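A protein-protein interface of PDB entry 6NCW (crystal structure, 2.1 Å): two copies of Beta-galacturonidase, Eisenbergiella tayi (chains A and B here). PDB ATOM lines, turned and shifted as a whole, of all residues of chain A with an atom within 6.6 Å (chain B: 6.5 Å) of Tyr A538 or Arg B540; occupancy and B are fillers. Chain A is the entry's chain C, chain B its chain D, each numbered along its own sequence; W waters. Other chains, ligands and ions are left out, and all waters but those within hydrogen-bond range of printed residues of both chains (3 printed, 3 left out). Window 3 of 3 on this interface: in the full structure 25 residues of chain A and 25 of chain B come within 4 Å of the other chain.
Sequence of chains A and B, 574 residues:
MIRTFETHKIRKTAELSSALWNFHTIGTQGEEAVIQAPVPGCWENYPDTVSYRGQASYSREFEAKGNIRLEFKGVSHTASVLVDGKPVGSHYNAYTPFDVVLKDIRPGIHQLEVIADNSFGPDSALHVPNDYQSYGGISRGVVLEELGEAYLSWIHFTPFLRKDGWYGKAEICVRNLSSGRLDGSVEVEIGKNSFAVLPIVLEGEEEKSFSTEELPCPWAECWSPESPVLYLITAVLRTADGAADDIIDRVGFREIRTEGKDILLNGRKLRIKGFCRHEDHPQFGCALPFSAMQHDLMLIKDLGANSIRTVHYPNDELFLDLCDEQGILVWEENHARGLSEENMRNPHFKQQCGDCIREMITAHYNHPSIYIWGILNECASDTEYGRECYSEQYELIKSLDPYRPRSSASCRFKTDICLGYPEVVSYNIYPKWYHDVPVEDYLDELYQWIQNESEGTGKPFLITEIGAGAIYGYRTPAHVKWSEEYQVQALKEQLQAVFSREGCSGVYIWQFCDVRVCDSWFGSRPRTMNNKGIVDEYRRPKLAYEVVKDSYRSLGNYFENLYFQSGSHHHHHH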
ATOM      1  N   HIS A 281     -19.343  -3.777  -2.846  1.00  0.00           N
ATOM      2  CA  HIS A 281     -20.015  -2.791  -2.012  1.00  0.00           C
ATOM      3  C   HIS A 281     -19.325  -2.869  -0.663  1.00  0.00           C
ATOM      4  O   HIS A 281     -18.959  -3.973  -0.242  1.00  0.00           O
ATOM      5  CB  HIS A 281     -21.509  -3.096  -1.889  1.00  0.00           C
ATOM      6  CG  HIS A 281     -22.304  -2.078  -1.128  1.00  0.00           C
ATOM      7  ND1 HIS A 281     -22.241  -1.950   0.243  1.00  0.00           N
ATOM      8  CD2 HIS A 281     -23.236  -1.184  -1.542  1.00  0.00           C
ATOM      9  CE1 HIS A 281     -23.079  -1.008   0.639  1.00  0.00           C
ATOM     10  NE2 HIS A 281     -23.690  -0.522  -0.425  1.00  0.00           N
ATOM     11  N   PRO A 282     -19.121  -1.749   0.030  1.00  0.00           N
ATOM     12  CA  PRO A 282     -18.342  -1.789   1.280  1.00  0.00           C
ATOM     13  C   PRO A 282     -19.051  -2.485   2.439  1.00  0.00           C
ATOM     14  O   PRO A 282     -18.376  -2.939   3.361  1.00  0.00           O
ATOM     15  CB  PRO A 282     -18.083  -0.298   1.588  1.00  0.00           C
ATOM     16  CG  PRO A 282     -19.031   0.447   0.767  1.00  0.00           C
ATOM     17  CD  PRO A 282     -19.372  -0.380  -0.435  1.00  0.00           C
ATOM     18  N   GLN A 283     -20.374  -2.580   2.445  1.00  0.00           N
ATOM     19  CA  GLN A 283     -21.040  -3.363   3.485  1.00  0.00           C
ATOM     20  C   GLN A 283     -21.364  -4.785   3.054  1.00  0.00           C
ATOM     21  O   GLN A 283     -21.505  -5.666   3.901  1.00  0.00           O
ATOM     22  CB  GLN A 283     -22.357  -2.712   3.913  1.00  0.00           C
ATOM     23  CG  GLN A 283     -22.289  -1.316   4.503  1.00  0.00           C
ATOM     24  CD  GLN A 283     -23.684  -0.870   4.935  1.00  0.00           C
ATOM     25  OE1 GLN A 283     -24.349  -0.081   4.251  1.00  0.00           O
ATOM     26  NE2 GLN A 283     -24.165  -1.444   6.029  1.00  0.00           N
ATOM     27  N   HIS A 295     -30.481   0.314  -6.459  1.00  0.00           N
ATOM     28  CA  HIS A 295     -29.905   1.634  -6.216  1.00  0.00           C
ATOM     29  C   HIS A 295     -28.808   1.931  -7.229  1.00  0.00           C
ATOM     30  O   HIS A 295     -28.820   2.983  -7.875  1.00  0.00           O
ATOM     31  CB  HIS A 295     -29.386   1.750  -4.783  1.00  0.00           C
ATOM     32  CG  HIS A 295     -29.068   3.155  -4.377  1.00  0.00           C
ATOM     33  ND1 HIS A 295     -27.778   3.644  -4.333  1.00  0.00           N
ATOM     34  CD2 HIS A 295     -29.873   4.188  -4.033  1.00  0.00           C
ATOM     35  CE1 HIS A 295     -27.803   4.913  -3.963  1.00  0.00           C
ATOM     36  NE2 HIS A 295     -29.061   5.269  -3.785  1.00  0.00           N
ATOM     37  N   CYS A 513     -18.176   2.291  -9.881  1.00  0.00           N
ATOM     38  CA  CYS A 513     -17.928   2.644  -8.490  1.00  0.00           C
ATOM     39  C   CYS A 513     -16.531   2.178  -8.101  1.00  0.00           C
ATOM     40  O   CYS A 513     -15.970   1.277  -8.720  1.00  0.00           O
ATOM     41  CB  CYS A 513     -18.988   2.021  -7.560  1.00  0.00           C
ATOM     42  SG  CYS A 513     -18.891   0.201  -7.464  1.00  0.00           S
ATOM     43  N   ASP A 514     -15.968   2.813  -7.072  1.00  0.00           N
ATOM     44  CA  ASP A 514     -14.703   2.361  -6.500  1.00  0.00           C
ATOM     45  C   ASP A 514     -14.884   0.974  -5.911  1.00  0.00           C
ATOM     46  O   ASP A 514     -15.938   0.651  -5.360  1.00  0.00           O
ATOM     47  CB  ASP A 514     -14.223   3.317  -5.398  1.00  0.00           C
ATOM     48  CG  ASP A 514     -13.920   4.720  -5.920  1.00  0.00           C
ATOM     49  OD1 ASP A 514     -13.815   4.911  -7.156  1.00  0.00           O
ATOM     50  OD2 ASP A 514     -13.791   5.642  -5.085  1.00  0.00           O
ATOM     51  N   ARG A 527      -5.653   3.542  -1.114  1.00  0.00           N
ATOM     52  CA  ARG A 527      -6.634   2.997  -0.179  1.00  0.00           C
ATOM     53  C   ARG A 527      -6.867   1.495  -0.361  1.00  0.00           C
ATOM     54  O   ARG A 527      -7.866   0.962   0.160  1.00  0.00           O
ATOM     55  CB  ARG A 527      -7.973   3.747  -0.306  1.00  0.00           C
ATOM     56  CG  ARG A 527      -7.847   5.290  -0.338  1.00  0.00           C
ATOM     57  CD  ARG A 527      -9.238   5.937  -0.409  1.00  0.00           C
ATOM     58  NE  ARG A 527      -9.983   5.513  -1.594  1.00  0.00           N
ATOM     59  CZ  ARG A 527     -11.285   5.277  -1.617  1.00  0.00           C
ATOM     60  NH1 ARG A 527     -12.017   5.406  -0.512  1.00  0.00           N
ATOM     61  NH2 ARG A 527     -11.860   4.906  -2.744  1.00  0.00           N
ATOM     62  N   VAL A 535     -18.837   7.098  -9.166  1.00  0.00           N
ATOM     63  CA  VAL A 535     -19.220   7.262  -7.775  1.00  0.00           C
ATOM     64  C   VAL A 535     -18.161   6.530  -6.955  1.00  0.00           C
ATOM     65  O   VAL A 535     -17.395   5.714  -7.483  1.00  0.00           O
ATOM     66  CB  VAL A 535     -20.658   6.757  -7.467  1.00  0.00           C
ATOM     67  CG1 VAL A 535     -21.679   7.566  -8.280  1.00  0.00           C
ATOM     68  CG2 VAL A 535     -20.827   5.234  -7.725  1.00  0.00           C
ATOM     69  N   ASP A 536     -18.065   6.880  -5.673  1.00  0.00           N
ATOM     70  CA  ASP A 536     -17.133   6.183  -4.792  1.00  0.00           C
ATOM     71  C   ASP A 536     -17.775   4.892  -4.257  1.00  0.00           C
ATOM     72  O   ASP A 536     -18.865   4.494  -4.681  1.00  0.00           O
ATOM     73  CB  ASP A 536     -16.622   7.132  -3.692  1.00  0.00           C
ATOM     74  CG  ASP A 536     -17.613   7.355  -2.550  1.00  0.00           C
ATOM     75  OD1 ASP A 536     -18.816   7.022  -2.674  1.00  0.00           O
ATOM     76  OD2 ASP A 536     -17.167   7.882  -1.497  1.00  0.00           O
ATOM     77  N   GLU A 537     -17.069   4.179  -3.362  1.00  0.00           N
ATOM     78  CA  GLU A 537     -17.571   2.879  -2.928  1.00  0.00           C
ATOM     79  C   GLU A 537     -18.906   3.017  -2.204  1.00  0.00           C
ATOM     80  O   GLU A 537     -19.698   2.076  -2.200  1.00  0.00           O
ATOM     81  CB  GLU A 537     -16.541   2.165  -2.044  1.00  0.00           C
ATOM     82  CG  GLU A 537     -16.199   2.863  -0.707  1.00  0.00           C
ATOM     83  CD  GLU A 537     -15.055   3.897  -0.832  1.00  0.00           C
ATOM     84  OE1 GLU A 537     -14.976   4.582  -1.878  1.00  0.00           O
ATOM     85  OE2 GLU A 537     -14.243   4.039   0.124  1.00  0.00           O
ATOM     86  N   TYR A 538     -19.178   4.185  -1.607  1.00  0.00           N
ATOM     87  CA  TYR A 538     -20.449   4.473  -0.940  1.00  0.00           C
ATOM     88  C   TYR A 538     -21.459   5.111  -1.869  1.00  0.00           C
ATOM     89  O   TYR A 538     -22.475   5.615  -1.385  1.00  0.00           O
ATOM     90  CB  TYR A 538     -20.239   5.384   0.286  1.00  0.00           C
ATOM     91  CG  TYR A 538     -19.367   4.704   1.322  1.00  0.00           C
ATOM     92  CD1 TYR A 538     -19.849   3.604   2.039  1.00  0.00           C
ATOM     93  CD2 TYR A 538     -18.053   5.098   1.526  1.00  0.00           C
ATOM     94  CE1 TYR A 538     -19.065   2.944   2.956  1.00  0.00           C
ATOM     95  CE2 TYR A 538     -17.246   4.428   2.445  1.00  0.00           C
ATOM     96  CZ  TYR A 538     -17.765   3.341   3.148  1.00  0.00           C
ATOM     97  OH  TYR A 538     -17.001   2.659   4.068  1.00  0.00           O
ATOM     98  N   ARG A 539     -21.185   5.111  -3.180  1.00  0.00           N
ATOM     99  CA  ARG A 539     -22.121   5.555  -4.208  1.00  0.00           C
ATOM    100  C   ARG A 539     -22.372   7.059  -4.157  1.00  0.00           C
ATOM    101  O   ARG A 539     -23.417   7.533  -4.599  1.00  0.00           O
ATOM    102  CB  ARG A 539     -23.443   4.783  -4.131  1.00  0.00           C
ATOM    103  CG  ARG A 539     -23.438   3.488  -4.942  1.00  0.00           C
ATOM    104  CD  ARG A 539     -22.506   2.430  -4.330  1.00  0.00           C
ATOM    105  NE  ARG A 539     -22.613   1.157  -5.043  1.00  0.00           N
ATOM    106  CZ  ARG A 539     -21.719   0.173  -4.968  1.00  0.00           C
ATOM    107  NH1 ARG A 539     -20.633   0.291  -4.209  1.00  0.00           N
ATOM    108  NH2 ARG A 539     -21.908  -0.934  -5.656  1.00  0.00           N
ATOM    109  N   ARG A 540     -21.418   7.804  -3.632  1.00  0.00           N
ATOM    110  CA  ARG A 540     -21.453   9.260  -3.656  1.00  0.00           C
ATOM    111  C   ARG A 540     -20.881   9.773  -4.973  1.00  0.00           C
ATOM    112  O   ARG A 540     -19.798   9.343  -5.374  1.00  0.00           O
ATOM    113  CB  ARG A 540     -20.654   9.818  -2.482  1.00  0.00           C
ATOM    114  CG  ARG A 540     -21.211   9.383  -1.124  1.00  0.00           C
ATOM    115  CD  ARG A 540     -20.404  10.037   0.026  1.00  0.00           C
ATOM    116  NE  ARG A 540     -19.073   9.451   0.135  1.00  0.00           N
ATOM    117  CZ  ARG A 540     -18.259   9.617   1.174  1.00  0.00           C
ATOM    118  NH1 ARG A 540     -18.648  10.343   2.218  1.00  0.00           N
ATOM    119  NH2 ARG A 540     -17.056   9.061   1.160  1.00  0.00           N
ATOM    120  N   PRO B 282     -28.142   5.829   4.429  1.00  0.00           N
ATOM    121  CA  PRO B 282     -27.944   6.797   3.323  1.00  0.00           C
ATOM    122  C   PRO B 282     -28.378   6.283   1.955  1.00  0.00           C
ATOM    123  O   PRO B 282     -28.736   7.087   1.088  1.00  0.00           O
ATOM    124  CB  PRO B 282     -26.431   7.078   3.366  1.00  0.00           C
ATOM    125  CG  PRO B 282     -25.846   5.944   4.185  1.00  0.00           C
ATOM    126  CD  PRO B 282     -26.899   5.494   5.137  1.00  0.00           C
ATOM    127  N   GLN B 283     -28.370   4.972   1.729  1.00  0.00           N
ATOM    128  CA  GLN B 283     -28.848   4.445   0.454  1.00  0.00           C
ATOM    129  C   GLN B 283     -30.312   4.034   0.492  1.00  0.00           C
ATOM    130  O   GLN B 283     -30.982   4.082  -0.548  1.00  0.00           O
ATOM    131  CB  GLN B 283     -28.024   3.229   0.013  1.00  0.00           C
ATOM    132  CG  GLN B 283     -26.667   3.551  -0.631  1.00  0.00           C
ATOM    133  CD  GLN B 283     -25.921   2.293  -1.074  1.00  0.00           C
ATOM    134  OE1 GLN B 283     -25.228   1.658  -0.279  1.00  0.00           O
ATOM    135  NE2 GLN B 283     -26.091   1.907  -2.340  1.00  0.00           N
ATOM    136  N   LEU B 299     -22.580  -5.283  13.896  1.00  0.00           N
ATOM    137  CA  LEU B 299     -21.832  -4.201  14.531  1.00  0.00           C
ATOM    138  C   LEU B 299     -22.276  -4.006  15.980  1.00  0.00           C
ATOM    139  O   LEU B 299     -21.449  -3.916  16.897  1.00  0.00           O
ATOM    140  CB  LEU B 299     -22.009  -2.907  13.731  1.00  0.00           C
ATOM    141  CG  LEU B 299     -21.405  -2.945  12.321  1.00  0.00           C
ATOM    142  CD1 LEU B 299     -21.737  -1.670  11.530  1.00  0.00           C
ATOM    143  CD2 LEU B 299     -19.902  -3.207  12.341  1.00  0.00           C
ATOM    144  N   TYR B 472     -17.650  12.486  11.785  1.00  0.00           N
ATOM    145  CA  TYR B 472     -16.657  11.514  11.353  1.00  0.00           C
ATOM    146  C   TYR B 472     -15.616  12.203  10.498  1.00  0.00           C
ATOM    147  O   TYR B 472     -15.951  12.842   9.496  1.00  0.00           O
ATOM    148  CB  TYR B 472     -17.314  10.378  10.555  1.00  0.00           C
ATOM    149  CG  TYR B 472     -16.330   9.332  10.067  1.00  0.00           C
ATOM    150  CD1 TYR B 472     -15.856   9.336   8.751  1.00  0.00           C
ATOM    151  CD2 TYR B 472     -15.827   8.376  10.940  1.00  0.00           C
ATOM    152  CE1 TYR B 472     -14.936   8.372   8.311  1.00  0.00           C
ATOM    153  CE2 TYR B 472     -14.895   7.430  10.525  1.00  0.00           C
ATOM    154  CZ  TYR B 472     -14.465   7.424   9.211  1.00  0.00           C
ATOM    155  OH  TYR B 472     -13.559   6.460   8.819  1.00  0.00           O
ATOM    156  N   ILE B 534     -22.275   6.288  17.005  1.00  0.00           N
ATOM    157  CA  ILE B 534     -20.999   5.664  17.305  1.00  0.00           C
ATOM    158  C   ILE B 534     -20.356   5.154  16.012  1.00  0.00           C
ATOM    159  O   ILE B 534     -19.132   5.065  15.917  1.00  0.00           O
ATOM    160  CB  ILE B 534     -21.200   4.554  18.357  1.00  0.00           C
ATOM    161  CG1 ILE B 534     -21.711   5.181  19.669  1.00  0.00           C
ATOM    162  CG2 ILE B 534     -19.929   3.723  18.557  1.00  0.00           C
ATOM    163  CD1 ILE B 534     -20.809   6.368  20.194  1.00  0.00           C
ATOM    164  N   VAL B 535     -21.157   4.823  15.011  1.00  0.00           N
ATOM    165  CA  VAL B 535     -20.706   4.711  13.634  1.00  0.00           C
ATOM    166  C   VAL B 535     -21.374   5.860  12.873  1.00  0.00           C
ATOM    167  O   VAL B 535     -22.394   6.415  13.309  1.00  0.00           O
ATOM    168  CB  VAL B 535     -21.042   3.327  13.019  1.00  0.00           C
ATOM    169  CG1 VAL B 535     -20.335   2.208  13.772  1.00  0.00           C
ATOM    170  CG2 VAL B 535     -22.563   3.071  12.979  1.00  0.00           C
ATOM    171  N   ASP B 536     -20.775   6.256  11.750  1.00  0.00           N
ATOM    172  CA  ASP B 536     -21.405   7.281  10.924  1.00  0.00           C
ATOM    173  C   ASP B 536     -22.513   6.657  10.051  1.00  0.00           C
ATOM    174  O   ASP B 536     -22.819   5.463  10.148  1.00  0.00           O
ATOM    175  CB  ASP B 536     -20.344   8.058  10.136  1.00  0.00           C
ATOM    176  CG  ASP B 536     -19.869   7.358   8.855  1.00  0.00           C
ATOM    177  OD1 ASP B 536     -20.154   6.167   8.621  1.00  0.00           O
ATOM    178  OD2 ASP B 536     -19.179   8.031   8.060  1.00  0.00           O
ATOM    179  N   GLU B 537     -23.146   7.473   9.201  1.00  0.00           N
ATOM    180  CA  GLU B 537     -24.267   6.974   8.408  1.00  0.00           C
ATOM    181  C   GLU B 537     -23.829   5.863   7.454  1.00  0.00           C
ATOM    182  O   GLU B 537     -24.628   4.979   7.121  1.00  0.00           O
ATOM    183  CB  GLU B 537     -24.941   8.130   7.658  1.00  0.00           C
ATOM    184  CG  GLU B 537     -24.123   8.797   6.535  1.00  0.00           C
ATOM    185  CD  GLU B 537     -23.219   9.927   7.041  1.00  0.00           C
ATOM    186  OE1 GLU B 537     -22.843   9.883   8.229  1.00  0.00           O
ATOM    187  OE2 GLU B 537     -22.897  10.875   6.260  1.00  0.00           O
ATOM    188  N   TYR B 538     -22.556   5.834   7.063  1.00  0.00           N
ATOM    189  CA  TYR B 538     -22.042   4.748   6.235  1.00  0.00           C
ATOM    190  C   TYR B 538     -21.543   3.563   7.054  1.00  0.00           C
ATOM    191  O   TYR B 538     -20.908   2.668   6.493  1.00  0.00           O
ATOM    192  CB  TYR B 538     -20.949   5.270   5.300  1.00  0.00           C
ATOM    193  CG  TYR B 538     -21.551   6.258   4.325  1.00  0.00           C
ATOM    194  CD1 TYR B 538     -22.418   5.813   3.336  1.00  0.00           C
ATOM    195  CD2 TYR B 538     -21.297   7.623   4.423  1.00  0.00           C
ATOM    196  CE1 TYR B 538     -23.009   6.692   2.444  1.00  0.00           C
ATOM    197  CE2 TYR B 538     -21.894   8.545   3.518  1.00  0.00           C
ATOM    198  CZ  TYR B 538     -22.754   8.049   2.532  1.00  0.00           C
ATOM    199  OH  TYR B 538     -23.371   8.881   1.637  1.00  0.00           O
ATOM    200  N   ARG B 539     -21.857   3.529   8.352  1.00  0.00           N
ATOM    201  CA  ARG B 539     -21.521   2.446   9.274  1.00  0.00           C
ATOM    202  C   ARG B 539     -20.016   2.345   9.541  1.00  0.00           C
ATOM    203  O   ARG B 539     -19.527   1.285   9.935  1.00  0.00           O
ATOM    204  CB  ARG B 539     -22.076   1.098   8.787  1.00  0.00           C
ATOM    205  CG  ARG B 539     -23.495   0.806   9.265  1.00  0.00           C
ATOM    206  CD  ARG B 539     -24.458   1.948   8.899  1.00  0.00           C
ATOM    207  NE  ARG B 539     -25.824   1.609   9.257  1.00  0.00           N
ATOM    208  CZ  ARG B 539     -26.885   2.401   9.077  1.00  0.00           C
ATOM    209  NH1 ARG B 539     -26.774   3.613   8.529  1.00  0.00           N
ATOM    210  NH2 ARG B 539     -28.072   1.975   9.459  1.00  0.00           N
ATOM    211  N   ARG B 540     -19.261   3.448   9.336  1.00  0.00           N
ATOM    212  CA  ARG B 540     -17.823   3.478   9.595  1.00  0.00           C
ATOM    213  C   ARG B 540     -17.577   3.802  11.068  1.00  0.00           C
ATOM    214  O   ARG B 540     -18.168   4.748  11.590  1.00  0.00           O
ATOM    215  CB  ARG B 540     -17.128   4.507   8.712  1.00  0.00           C
ATOM    216  CG  ARG B 540     -17.280   4.223   7.226  1.00  0.00           C
ATOM    217  CD  ARG B 540     -16.519   5.235   6.371  1.00  0.00           C
ATOM    218  NE  ARG B 540     -17.149   6.554   6.402  1.00  0.00           N
ATOM    219  CZ  ARG B 540     -16.841   7.556   5.591  1.00  0.00           C
ATOM    220  NH1 ARG B 540     -15.908   7.391   4.665  1.00  0.00           N
ATOM    221  NH2 ARG B 540     -17.452   8.731   5.724  1.00  0.00           N
ATOM    222  N   PRO B 541     -16.772   3.022  11.782  1.00  0.00           N
ATOM    223  CA  PRO B 541     -16.636   3.254  13.231  1.00  0.00           C
ATOM    224  C   PRO B 541     -15.879   4.545  13.522  1.00  0.00           C
ATOM    225  O   PRO B 541     -14.796   4.777  12.980  1.00  0.00           O
ATOM    226  CB  PRO B 541     -15.873   2.020  13.725  1.00  0.00           C
ATOM    227  CG  PRO B 541     -15.344   1.329  12.481  1.00  0.00           C
ATOM    228  CD  PRO B 541     -16.160   1.763  11.324  1.00  0.00           C
ATOM    229  N   LYS B 542     -16.472   5.400  14.364  1.00  0.00           N
ATOM    230  CA  LYS B 542     -15.793   6.568  14.915  1.00  0.00           C
ATOM    231  C   LYS B 542     -14.797   6.144  16.004  1.00  0.00           C
ATOM    232  O   LYS B 542     -14.805   5.002  16.486  1.00  0.00           O
ATOM    233  CB  LYS B 542     -16.810   7.560  15.490  1.00  0.00           C
ATOM    234  CG  LYS B 542     -17.771   8.129  14.446  1.00  0.00           C
ATOM    235  CD  LYS B 542     -18.725   9.163  15.003  1.00  0.00           C
ATOM    236  CE  LYS B 542     -19.886   9.382  14.012  1.00  0.00           C
ATOM    237  NZ  LYS B 542     -20.951  10.204  14.650  1.00  0.00           N
ATOM    238  N   TYR B 545     -16.034   4.259  18.990  1.00  0.00           N
ATOM    239  CA  TYR B 545     -16.448   2.867  18.853  1.00  0.00           C
ATOM    240  C   TYR B 545     -15.674   1.955  19.804  1.00  0.00           C
ATOM    241  O   TYR B 545     -16.264   1.082  20.449  1.00  0.00           O
ATOM    242  CB  TYR B 545     -16.271   2.437  17.402  1.00  0.00           C
ATOM    243  CG  TYR B 545     -16.763   1.065  17.022  1.00  0.00           C
ATOM    244  CD1 TYR B 545     -16.013  -0.078  17.307  1.00  0.00           C
ATOM    245  CD2 TYR B 545     -17.937   0.919  16.307  1.00  0.00           C
ATOM    246  CE1 TYR B 545     -16.439  -1.312  16.924  1.00  0.00           C
ATOM    247  CE2 TYR B 545     -18.377  -0.324  15.910  1.00  0.00           C
ATOM    248  CZ  TYR B 545     -17.627  -1.434  16.223  1.00  0.00           C
ATOM    249  OH  TYR B 545     -18.076  -2.656  15.830  1.00  0.00           O
HETATM  250  O   HOH W   1     -25.562  -0.040  -4.102  1.00  0.00           O
HETATM  251  O   HOH W   2     -26.763  -1.184   7.402  1.00  0.00           O
HETATM  252  O   HOH W   3     -18.602   1.193   5.986  1.00  0.00           O
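The side-chain amide nitrogen (NE2) of Gln B283 sits at hydrogen-bond distance from a ring nitrogen (ND1) of His A295.
The side-chain amide oxygen (OE1) of Gln B283 sits at hydrogen-bond distance from a ring nitrogen (NE2) of His A281.
The backbone NH (N) of Gln A283 sits at hydrogen-bond distance from a ring nitrogen (ND1) of His A281.
The side-chain carboxylate (OD1) of Asp A536 lies within hydrogen-bond range of the backbone NH (N) of Tyr A538.
The guanidinium group (NH2) of Arg A540 lies within salt-bridge range of the side-chain carboxylate (OD2) of Asp A536 (2.9 Å).
The side-chain carboxylate of Asp B536 is in salt-bridge range of the guanidinium group of Arg B540.
The side-chain carboxylate (OD1) of Asp B536 is in hydrogen-bond range of the backbone NH (N) of Arg B539.
O of Glu B537 is in hydrogen-bond range of NH1 of Arg B539 (2.9 Å).
Gln A283 touches Arg B539 (NE2 to CG, 3.998 Å).
Tyr B538 touches Tyr A538 (CD1 to CD1, 3.6 Å).
Tyr A538 touches Arg B540.
Arg A540 touches Tyr B538 (CG to OH, 3.5 Å).
Printed residues of chain B within 4 Å of Gln A283: Arg B539.
Printed residues of chain B within 4 Å of His A295: Gln B283.
Val A535 touches none of the printed residues of chain B.
Tyr A538 touches two residues of chain B.
Arg B540 touches just one residue of chain A: Tyr A538 (3.5 Å).
The nearest residue of chain B that does not touch Tyr A538 is Gln B283 (4.7 Å).
The nearest printed residue of chain A that does not touch Tyr B538 is Gln A283 (4.7 Å).
Hydrophobic or aromatic side chains of chain B that line the printed part of chain A: Tyr B538.
Of the 13 printed residues of chain A, 5 touch a printed residue of chain B.
Printed residues of chain A that touch a printed residue of chain B: His A281, Gln A283, His A295, Tyr A538 and Arg A540.
Hydrophobic or aromatic side chains of chain A that line the printed part of chain B: His A281, His A295 and Tyr A538.
Along chain A the printed residues that touch a printed residue of chain B span positions 281 to 540.
Among the printed residues, 6 pairs touch across the chains.
Among the printed residues, no Asp or Glu carboxylate lies within 4 Å of a Lys or Arg side-chain nitrogen of the other chain.
Gln A283 touches Arg B539, but with the chains exchanged Arg A539 does not touch Gln B283 (4.04 Å).
Tyr B538 touches its own counterpart, Tyr A538.
Tyr A538 touches Arg B540, and with the chains exchanged Arg A540 touches Tyr B538.
Water W1 bridges the side-chain amide nitrogen (NE2) of Gln B283 (2.7 Å) and the guanidinium group (NE) of Arg A539 (3.3 Å).
Water W3 bridges the backbone carbonyl oxygen of Tyr B538 (2.8 Å) and the side-chain hydroxyl of Tyr A538 (2.9 Å).
Water W2 lies within hydrogen-bond range of the side-chain amide nitrogen of Gln A283 and the guanidinium group of Arg B539.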
